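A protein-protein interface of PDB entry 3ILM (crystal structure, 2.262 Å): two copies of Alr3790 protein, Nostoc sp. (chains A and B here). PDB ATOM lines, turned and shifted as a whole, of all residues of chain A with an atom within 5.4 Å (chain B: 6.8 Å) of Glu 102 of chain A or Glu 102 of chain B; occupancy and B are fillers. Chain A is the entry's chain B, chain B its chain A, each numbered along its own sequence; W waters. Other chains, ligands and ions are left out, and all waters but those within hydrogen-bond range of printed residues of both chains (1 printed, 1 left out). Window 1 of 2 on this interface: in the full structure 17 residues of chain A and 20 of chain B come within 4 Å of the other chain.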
ATOM      1  N   TYR A  29      19.057 -25.269  40.201  1.00  0.00           N
ATOM      2  CA  TYR A  29      20.063 -25.592  39.201  1.00  0.00           C
ATOM      3  C   TYR A  29      19.500 -25.309  37.812  1.00  0.00           C
ATOM      4  O   TYR A  29      20.107 -24.582  37.022  1.00  0.00           O
ATOM      5  CB  TYR A  29      20.437 -27.068  39.282  1.00  0.00           C
ATOM      6  CG  TYR A  29      21.369 -27.540  38.176  1.00  0.00           C
ATOM      7  CD1 TYR A  29      22.761 -27.501  38.334  1.00  0.00           C
ATOM      8  CD2 TYR A  29      20.861 -28.029  36.974  1.00  0.00           C
ATOM      9  CE1 TYR A  29      23.611 -27.941  37.326  1.00  0.00           C
ATOM     10  CE2 TYR A  29      21.706 -28.471  35.964  1.00  0.00           C
ATOM     11  CZ  TYR A  29      23.074 -28.424  36.148  1.00  0.00           C
ATOM     12  OH  TYR A  29      23.906 -28.881  35.152  1.00  0.00           O
ATOM     13  N   ASN A  30      18.337 -25.901  37.533  1.00  0.00           N
ATOM     14  CA  ASN A  30      17.664 -25.758  36.245  1.00  0.00           C
ATOM     15  C   ASN A  30      17.409 -24.308  35.872  1.00  0.00           C
ATOM     16  O   ASN A  30      17.455 -23.954  34.692  1.00  0.00           O
ATOM     17  CB  ASN A  30      16.329 -26.506  36.243  1.00  0.00           C
ATOM     18  CG  ASN A  30      16.495 -28.014  36.209  1.00  0.00           C
ATOM     19  OD1 ASN A  30      17.440 -28.537  35.629  1.00  0.00           O
ATOM     20  ND2 ASN A  30      15.553 -28.721  36.813  1.00  0.00           N
ATOM     21  N   ASP A  31      17.126 -23.472  36.868  1.00  0.00           N
ATOM     22  CA  ASP A  31      16.872 -22.068  36.602  1.00  0.00           C
ATOM     23  C   ASP A  31      18.156 -21.306  36.286  1.00  0.00           C
ATOM     24  O   ASP A  31      18.127 -20.231  35.691  1.00  0.00           O
ATOM     25  CB  ASP A  31      16.139 -21.434  37.785  1.00  0.00           C
ATOM     26  CG  ASP A  31      14.629 -21.603  37.685  1.00  0.00           C
ATOM     27  OD1 ASP A  31      14.174 -22.739  37.441  1.00  0.00           O
ATOM     28  OD2 ASP A  31      13.897 -20.604  37.845  1.00  0.00           O
ATOM     29  N   GLY A  32      19.291 -21.872  36.668  1.00  0.00           N
ATOM     30  CA  GLY A  32      20.543 -21.201  36.385  1.00  0.00           C
ATOM     31  C   GLY A  32      21.689 -21.767  37.178  1.00  0.00           C
ATOM     32  O   GLY A  32      21.647 -21.784  38.411  1.00  0.00           O
ATOM     33  N   HIS A  33      22.708 -22.252  36.475  1.00  0.00           N
ATOM     34  CA  HIS A  33      23.890 -22.798  37.128  1.00  0.00           C
ATOM     35  C   HIS A  33      25.127 -22.309  36.396  1.00  0.00           C
ATOM     36  O   HIS A  33      25.025 -21.733  35.308  1.00  0.00           O
ATOM     37  CB  HIS A  33      23.853 -24.340  37.154  1.00  0.00           C
ATOM     38  CG  HIS A  33      23.599 -24.974  35.820  1.00  0.00           C
ATOM     39  ND1 HIS A  33      22.330 -25.252  35.354  1.00  0.00           N
ATOM     40  CD2 HIS A  33      24.451 -25.381  34.846  1.00  0.00           C
ATOM     41  CE1 HIS A  33      22.412 -25.796  34.152  1.00  0.00           C
ATOM     42  NE2 HIS A  33      23.688 -25.885  33.819  1.00  0.00           N
ATOM     43  N   ILE A  34      26.296 -22.518  36.987  1.00  0.00           N
ATOM     44  CA  ILE A  34      27.522 -22.093  36.337  1.00  0.00           C
ATOM     45  C   ILE A  34      27.678 -22.998  35.123  1.00  0.00           C
ATOM     46  O   ILE A  34      27.417 -24.203  35.213  1.00  0.00           O
ATOM     47  CB  ILE A  34      28.726 -22.247  37.266  1.00  0.00           C
ATOM     48  CG1 ILE A  34      28.575 -21.291  38.449  1.00  0.00           C
ATOM     49  CG2 ILE A  34      30.020 -21.994  36.488  1.00  0.00           C
ATOM     50  CD1 ILE A  34      29.665 -21.418  39.471  1.00  0.00           C
ATOM     51  N   MET A  35      28.078 -22.416  33.991  1.00  0.00           N
ATOM     52  CA  MET A  35      28.226 -23.175  32.749  1.00  0.00           C
ATOM     53  C   MET A  35      29.111 -24.410  32.857  1.00  0.00           C
ATOM     54  O   MET A  35      30.277 -24.322  33.212  1.00  0.00           O
ATOM     55  CB  MET A  35      28.761 -22.273  31.638  1.00  0.00           C
ATOM     56  CG  MET A  35      28.643 -22.882  30.241  1.00  0.00           C
ATOM     57  SD  MET A  35      29.381 -21.715  28.872  1.00  0.00           S
ATOM     58  CE  MET A  35      28.016 -20.380  28.860  1.00  0.00           C
ATOM     59  N   GLY A  36      28.550 -25.565  32.531  1.00  0.00           N
ATOM     60  CA  GLY A  36      29.317 -26.794  32.599  1.00  0.00           C
ATOM     61  C   GLY A  36      29.142 -27.551  33.902  1.00  0.00           C
ATOM     62  O   GLY A  36      29.546 -28.704  34.005  1.00  0.00           O
ATOM     63  N   ALA A  37      28.533 -26.908  34.893  1.00  0.00           N
ATOM     64  CA  ALA A  37      28.314 -27.528  36.193  1.00  0.00           C
ATOM     65  C   ALA A  37      27.429 -28.765  36.124  1.00  0.00           C
ATOM     66  O   ALA A  37      26.501 -28.837  35.325  1.00  0.00           O
ATOM     67  CB  ALA A  37      27.693 -26.514  37.158  1.00  0.00           C
ATOM     68  N   PRO A 100      29.705 -16.875  32.709  1.00  0.00           N
ATOM     69  CA  PRO A 100      28.498 -17.175  31.939  1.00  0.00           C
ATOM     70  C   PRO A 100      27.669 -18.293  32.597  1.00  0.00           C
ATOM     71  O   PRO A 100      28.204 -19.306  33.065  1.00  0.00           O
ATOM     72  CB  PRO A 100      29.055 -17.587  30.589  1.00  0.00           C
ATOM     73  CG  PRO A 100      30.292 -18.336  30.990  1.00  0.00           C
ATOM     74  CD  PRO A 100      30.901 -17.443  32.060  1.00  0.00           C
ATOM     75  N   THR A 101      26.357 -18.090  32.612  1.00  0.00           N
ATOM     76  CA  THR A 101      25.427 -19.024  33.213  1.00  0.00           C
ATOM     77  C   THR A 101      24.726 -19.909  32.182  1.00  0.00           C
ATOM     78  O   THR A 101      24.722 -19.607  30.995  1.00  0.00           O
ATOM     79  CB  THR A 101      24.398 -18.245  34.038  1.00  0.00           C
ATOM     80  OG1 THR A 101      25.053 -17.688  35.183  1.00  0.00           O
ATOM     81  CG2 THR A 101      23.269 -19.142  34.493  1.00  0.00           C
ATOM     82  N   GLU A 102      24.147 -21.013  32.649  1.00  0.00           N
ATOM     83  CA  GLU A 102      23.442 -21.967  31.799  1.00  0.00           C
ATOM     84  C   GLU A 102      22.130 -22.270  32.513  1.00  0.00           C
ATOM     85  O   GLU A 102      22.134 -22.583  33.705  1.00  0.00           O
ATOM     86  CB  GLU A 102      24.265 -23.259  31.665  1.00  0.00           C
ATOM     87  CG  GLU A 102      23.811 -24.234  30.569  1.00  0.00           C
ATOM     88  CD  GLU A 102      24.193 -25.706  30.860  1.00  0.00           C
ATOM     89  OE1 GLU A 102      25.369 -25.984  31.182  1.00  0.00           O
ATOM     90  OE2 GLU A 102      23.312 -26.588  30.764  1.00  0.00           O
ATOM     91  N   GLY A 103      21.016 -22.173  31.789  1.00  0.00           N
ATOM     92  CA  GLY A 103      19.718 -22.448  32.381  1.00  0.00           C
ATOM     93  C   GLY A 103      18.789 -23.293  31.524  1.00  0.00           C
ATOM     94  O   GLY A 103      18.823 -23.213  30.300  1.00  0.00           O
ATOM     95  N   ILE A 104      17.952 -24.100  32.178  1.00  0.00           N
ATOM     96  CA  ILE A 104      16.991 -24.969  31.493  1.00  0.00           C
ATOM     97  C   ILE A 104      15.682 -24.229  31.234  1.00  0.00           C
ATOM     98  O   ILE A 104      15.372 -23.248  31.904  1.00  0.00           O
ATOM     99  CB  ILE A 104      16.699 -26.256  32.332  1.00  0.00           C
ATOM    100  CG1 ILE A 104      17.722 -27.346  32.011  1.00  0.00           C
ATOM    101  CG2 ILE A 104      15.312 -26.791  32.032  1.00  0.00           C
ATOM    102  CD1 ILE A 104      19.156 -27.009  32.355  1.00  0.00           C
ATOM    103  N   ILE A 105      14.924 -24.695  30.247  1.00  0.00           N
ATOM    104  CA  ILE A 105      13.637 -24.093  29.902  1.00  0.00           C
ATOM    105  C   ILE A 105      12.705 -25.168  29.330  1.00  0.00           C
ATOM    106  O   ILE A 105      11.849 -25.711  30.035  1.00  0.00           O
ATOM    107  CB  ILE A 105      13.797 -22.955  28.849  1.00  0.00           C
ATOM    108  CG1 ILE A 105      14.908 -21.987  29.274  1.00  0.00           C
ATOM    109  CG2 ILE A 105      12.491 -22.188  28.716  1.00  0.00           C
ATOM    110  CD1 ILE A 105      15.212 -20.911  28.248  1.00  0.00           C
ATOM    111  N   TYR B  29      22.586 -20.265  19.027  1.00  0.00           N
ATOM    112  CA  TYR B  29      22.721 -21.472  19.832  1.00  0.00           C
ATOM    113  C   TYR B  29      22.624 -21.070  21.287  1.00  0.00           C
ATOM    114  O   TYR B  29      21.854 -21.655  22.050  1.00  0.00           O
ATOM    115  CB  TYR B  29      24.091 -22.110  19.577  1.00  0.00           C
ATOM    116  CG  TYR B  29      24.531 -23.171  20.584  1.00  0.00           C
ATOM    117  CD1 TYR B  29      24.139 -24.499  20.442  1.00  0.00           C
ATOM    118  CD2 TYR B  29      25.366 -22.841  21.657  1.00  0.00           C
ATOM    119  CE1 TYR B  29      24.569 -25.481  21.332  1.00  0.00           C
ATOM    120  CE2 TYR B  29      25.798 -23.815  22.564  1.00  0.00           C
ATOM    121  CZ  TYR B  29      25.392 -25.137  22.388  1.00  0.00           C
ATOM    122  OH  TYR B  29      25.806 -26.120  23.253  1.00  0.00           O
ATOM    123  N   ASN B  30      23.410 -20.056  21.649  1.00  0.00           N
ATOM    124  CA  ASN B  30      23.475 -19.535  23.012  1.00  0.00           C
ATOM    125  C   ASN B  30      22.156 -19.045  23.553  1.00  0.00           C
ATOM    126  O   ASN B  30      21.852 -19.243  24.728  1.00  0.00           O
ATOM    127  CB  ASN B  30      24.494 -18.402  23.098  1.00  0.00           C
ATOM    128  CG  ASN B  30      25.920 -18.906  23.200  1.00  0.00           C
ATOM    129  OD1 ASN B  30      26.872 -18.135  23.055  1.00  0.00           O
ATOM    130  ND2 ASN B  30      26.080 -20.201  23.463  1.00  0.00           N
ATOM    131  N   ASP B  31      21.362 -18.397  22.712  1.00  0.00           N
ATOM    132  CA  ASP B  31      20.082 -17.897  23.181  1.00  0.00           C
ATOM    133  C   ASP B  31      19.148 -19.068  23.432  1.00  0.00           C
ATOM    134  O   ASP B  31      18.191 -18.963  24.198  1.00  0.00           O
ATOM    135  CB  ASP B  31      19.462 -16.928  22.166  1.00  0.00           C
ATOM    136  CG  ASP B  31      20.296 -15.673  21.972  1.00  0.00           C
ATOM    137  OD1 ASP B  31      20.965 -15.243  22.938  1.00  0.00           O
ATOM    138  OD2 ASP B  31      20.270 -15.104  20.859  1.00  0.00           O
ATOM    139  N   GLY B  32      19.431 -20.197  22.799  1.00  0.00           N
ATOM    140  CA  GLY B  32      18.583 -21.348  23.018  1.00  0.00           C
ATOM    141  C   GLY B  32      18.886 -22.503  22.107  1.00  0.00           C
ATOM    142  O   GLY B  32      18.927 -22.333  20.892  1.00  0.00           O
ATOM    143  N   HIS B  33      19.110 -23.677  22.691  1.00  0.00           N
ATOM    144  CA  HIS B  33      19.390 -24.874  21.909  1.00  0.00           C
ATOM    145  C   HIS B  33      18.835 -26.102  22.595  1.00  0.00           C
ATOM    146  O   HIS B  33      18.482 -26.052  23.779  1.00  0.00           O
ATOM    147  CB  HIS B  33      20.898 -25.065  21.688  1.00  0.00           C
ATOM    148  CG  HIS B  33      21.693 -25.203  22.948  1.00  0.00           C
ATOM    149  ND1 HIS B  33      22.220 -24.121  23.619  1.00  0.00           N
ATOM    150  CD2 HIS B  33      22.084 -26.300  23.639  1.00  0.00           C
ATOM    151  CE1 HIS B  33      22.907 -24.547  24.666  1.00  0.00           C
ATOM    152  NE2 HIS B  33      22.838 -25.865  24.698  1.00  0.00           N
ATOM    153  N   ILE B  34      18.759 -27.196  21.842  1.00  0.00           N
ATOM    154  CA  ILE B  34      18.258 -28.463  22.349  1.00  0.00           C
ATOM    155  C   ILE B  34      19.192 -28.946  23.445  1.00  0.00           C
ATOM    156  O   ILE B  34      20.419 -28.867  23.320  1.00  0.00           O
ATOM    157  CB  ILE B  34      18.164 -29.513  21.220  1.00  0.00           C
ATOM    158  CG1 ILE B  34      17.081 -29.081  20.223  1.00  0.00           C
ATOM    159  CG2 ILE B  34      17.842 -30.900  21.800  1.00  0.00           C
ATOM    160  CD1 ILE B  34      16.961 -29.971  19.009  1.00  0.00           C
ATOM    161  N   MET B  35      18.604 -29.417  24.537  1.00  0.00           N
ATOM    162  CA  MET B  35      19.390 -29.887  25.664  1.00  0.00           C
ATOM    163  C   MET B  35      20.416 -30.936  25.242  1.00  0.00           C
ATOM    164  O   MET B  35      20.046 -31.990  24.726  1.00  0.00           O
ATOM    165  CB  MET B  35      18.463 -30.466  26.729  1.00  0.00           C
ATOM    166  CG  MET B  35      19.196 -31.111  27.898  1.00  0.00           C
ATOM    167  SD  MET B  35      18.041 -31.300  29.448  1.00  0.00           S
ATOM    168  CE  MET B  35      17.887 -29.425  29.837  1.00  0.00           C
ATOM    169  N   GLY B  36      21.701 -30.648  25.463  1.00  0.00           N
ATOM    170  CA  GLY B  36      22.751 -31.590  25.102  1.00  0.00           C
ATOM    171  C   GLY B  36      23.437 -31.325  23.764  1.00  0.00           C
ATOM    172  O   GLY B  36      24.551 -31.812  23.523  1.00  0.00           O
ATOM    173  N   ALA B  37      22.788 -30.554  22.889  1.00  0.00           N
ATOM    174  CA  ALA B  37      23.374 -30.244  21.586  1.00  0.00           C
ATOM    175  C   ALA B  37      24.704 -29.519  21.691  1.00  0.00           C
ATOM    176  O   ALA B  37      24.936 -28.745  22.620  1.00  0.00           O
ATOM    177  CB  ALA B  37      22.407 -29.404  20.746  1.00  0.00           C
ATOM    178  N   PRO B 100      13.096 -30.150  26.424  1.00  0.00           N
ATOM    179  CA  PRO B 100      13.775 -29.066  27.139  1.00  0.00           C
ATOM    180  C   PRO B 100      14.715 -28.235  26.270  1.00  0.00           C
ATOM    181  O   PRO B 100      15.334 -28.745  25.341  1.00  0.00           O
ATOM    182  CB  PRO B 100      14.552 -29.801  28.233  1.00  0.00           C
ATOM    183  CG  PRO B 100      13.779 -31.052  28.427  1.00  0.00           C
ATOM    184  CD  PRO B 100      13.432 -31.449  27.027  1.00  0.00           C
ATOM    185  N   THR B 101      14.828 -26.954  26.592  1.00  0.00           N
ATOM    186  CA  THR B 101      15.709 -26.067  25.868  1.00  0.00           C
ATOM    187  C   THR B 101      16.603 -25.344  26.852  1.00  0.00           C
ATOM    188  O   THR B 101      16.116 -24.761  27.817  1.00  0.00           O
ATOM    189  CB  THR B 101      14.917 -25.032  25.069  1.00  0.00           C
ATOM    190  OG1 THR B 101      14.427 -25.641  23.869  1.00  0.00           O
ATOM    191  CG2 THR B 101      15.795 -23.844  24.723  1.00  0.00           C
ATOM    192  N   GLU B 102      17.910 -25.386  26.616  1.00  0.00           N
ATOM    193  CA  GLU B 102      18.842 -24.703  27.498  1.00  0.00           C
ATOM    194  C   GLU B 102      19.454 -23.476  26.811  1.00  0.00           C
ATOM    195  O   GLU B 102      19.631 -23.444  25.590  1.00  0.00           O
ATOM    196  CB  GLU B 102      19.938 -25.670  27.979  1.00  0.00           C
ATOM    197  CG  GLU B 102      20.786 -26.301  26.881  1.00  0.00           C
ATOM    198  CD  GLU B 102      21.722 -27.402  27.391  1.00  0.00           C
ATOM    199  OE1 GLU B 102      22.613 -27.827  26.619  1.00  0.00           O
ATOM    200  OE2 GLU B 102      21.558 -27.846  28.554  1.00  0.00           O
ATOM    201  N   GLY B 103      19.751 -22.453  27.603  1.00  0.00           N
ATOM    202  CA  GLY B 103      20.335 -21.245  27.053  1.00  0.00           C
ATOM    203  C   GLY B 103      21.464 -20.714  27.909  1.00  0.00           C
ATOM    204  O   GLY B 103      21.480 -20.901  29.127  1.00  0.00           O
ATOM    205  N   ILE B 104      22.408 -20.049  27.252  1.00  0.00           N
ATOM    206  CA  ILE B 104      23.572 -19.460  27.905  1.00  0.00           C
ATOM    207  C   ILE B 104      23.348 -17.969  28.151  1.00  0.00           C
ATOM    208  O   ILE B 104      22.654 -17.308  27.379  1.00  0.00           O
ATOM    209  CB  ILE B 104      24.843 -19.648  27.039  1.00  0.00           C
ATOM    210  CG1 ILE B 104      25.372 -21.079  27.177  1.00  0.00           C
ATOM    211  CG2 ILE B 104      25.897 -18.646  27.433  1.00  0.00           C
ATOM    212  CD1 ILE B 104      24.722 -22.092  26.266  1.00  0.00           C
ATOM    213  N   ILE B 105      23.948 -17.445  29.220  1.00  0.00           N
ATOM    214  CA  ILE B 105      23.789 -16.041  29.584  1.00  0.00           C
ATOM    215  C   ILE B 105      25.095 -15.423  30.080  1.00  0.00           C
ATOM    216  O   ILE B 105      25.292 -14.202  30.002  1.00  0.00           O
ATOM    217  CB  ILE B 105      22.730 -15.898  30.688  1.00  0.00           C
ATOM    218  CG1 ILE B 105      21.573 -16.860  30.421  1.00  0.00           C
ATOM    219  CG2 ILE B 105      22.195 -14.476  30.720  1.00  0.00           C
ATOM    220  CD1 ILE B 105      20.524 -16.874  31.518  1.00  0.00           C
HETATM  221  O   HOH W   1      24.768 -28.115  28.966  1.00  0.00           O
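Among the printed residues, merely in contact across the chains: Ile 104 of chain A with Met 35 of chain B, Met 35 of chain A with Ile 104 of chain B, Gly 103 of chain A with Glu 102 of chain B, Thr 101 of chain A with Ile 104 of chain B, Glu 102 of chain A with Gly 103 of chain B, Ile 104 of chain A with Thr 101 of chain B, Thr 101 of chain A with Gly 103 of chain B and Gly 103 of chain A with Thr 101 of chain B.
Glu 102 of chain A touches just these residues of chain B: Glu 102 and Gly 103. Of the printed residues of chain A, Met 35 of chain B touches Ile 104. Of chain A, only Glu 102 (3.1 Å) and Gly 103 (3.2 Å) come within 4 Å of Glu 102 of chain B. Of the printed residues of chain A, Ile 104 of chain B touches Met 35 (3.1 Å) and Thr 101 (3.3 Å). The nearest residue of chain B that does not touch Glu 102 of chain A is Ile 104 of chain B (4.6 Å). The nearest residue of chain A that does not touch Glu 102 of chain B is Ile 104 of chain A (4.4 Å).
Met 35 of chain A touches Ile 104 of chain B, and with the chains exchanged Ile 104 of chain A touches Met 35 of chain B. Thr 101 of chain A touches Gly 103 of chain B, and with the chains exchanged Gly 103 of chain A touches Thr 101 of chain B. Thr 101 of chain A touches Ile 104 of chain B, and with the chains exchanged Ile 104 of chain A touches Thr 101 of chain B. Glu 102 of chain A touches Gly 103 of chain B, and with the chains exchanged Gly 103 of chain A touches Glu 102 of chain B.
O of Thr 101 of chain B sits at hydrogen-bond distance from N of Ile 105 of chain A (2.7 Å). The backbone NH (N) of Gly 103 of chain B lies within hydrogen-bond range of the backbone carbonyl oxygen (O) of Gly 103 of chain A. The backbone carbonyl oxygen of Thr 101 of chain A sits at hydrogen-bond distance from the backbone NH of Ile 105 of chain B (2.9 Å). OE2 of Glu 102 of chain A sits close to OE2 of Glu 102 of chain B, 3.1 Å away.
The backbone carbonyl oxygen (O) of Asn 30 of chain B lies within hydrogen-bond range of the backbone NH (N) of Ile 104 of chain B, at 2.7 Å. The backbone NH (N) of Met 35 of chain B is in hydrogen-bond range of the backbone carbonyl oxygen (O) of Pro 100 of chain B, 3.4 Å away. The backbone carbonyl oxygen of Asn 30 of chain A sits at hydrogen-bond distance from the backbone NH of Ile 104 of chain A (2.6 Å). O of Glu 102 of chain A lies within hydrogen-bond range of N of His 33 of chain A. The backbone NH (N) of Met 35 of chain A is in hydrogen-bond range of the backbone carbonyl oxygen (O) of Pro 100 of chain A, 3.2 Å away. N of Gly 36 of chain A is in hydrogen-bond range of OE1 of Glu 102 of chain A (3.5 Å).
Of the 15 printed residues of chain A, 6 touch a printed residue of chain B. Printed residues of chain A that touch a printed residue of chain B: Met 35, Thr 101, Glu 102, Gly 103, Ile 104 and Ile 105. Hydrophobic or aromatic side chains of chain A that line the printed part of chain B: Met 35, Ile 104 and Ile 105. Of the 15 printed residues of chain B, 6 touch a printed residue of chain A. Hydrophobic or aromatic side chains of chain B within 4 Å of the printed part of chain A: Met 35 and Ile 104. Among the printed residues, no Asp or Glu carboxylate lies within 4 Å of a Lys or Arg side-chain nitrogen of the other chain.
Water W1 lies within hydrogen-bond range of OE2 of Glu 102 of chain A (2.8 Å) and OE2 of Glu 102 of chain B (3.2 Å).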
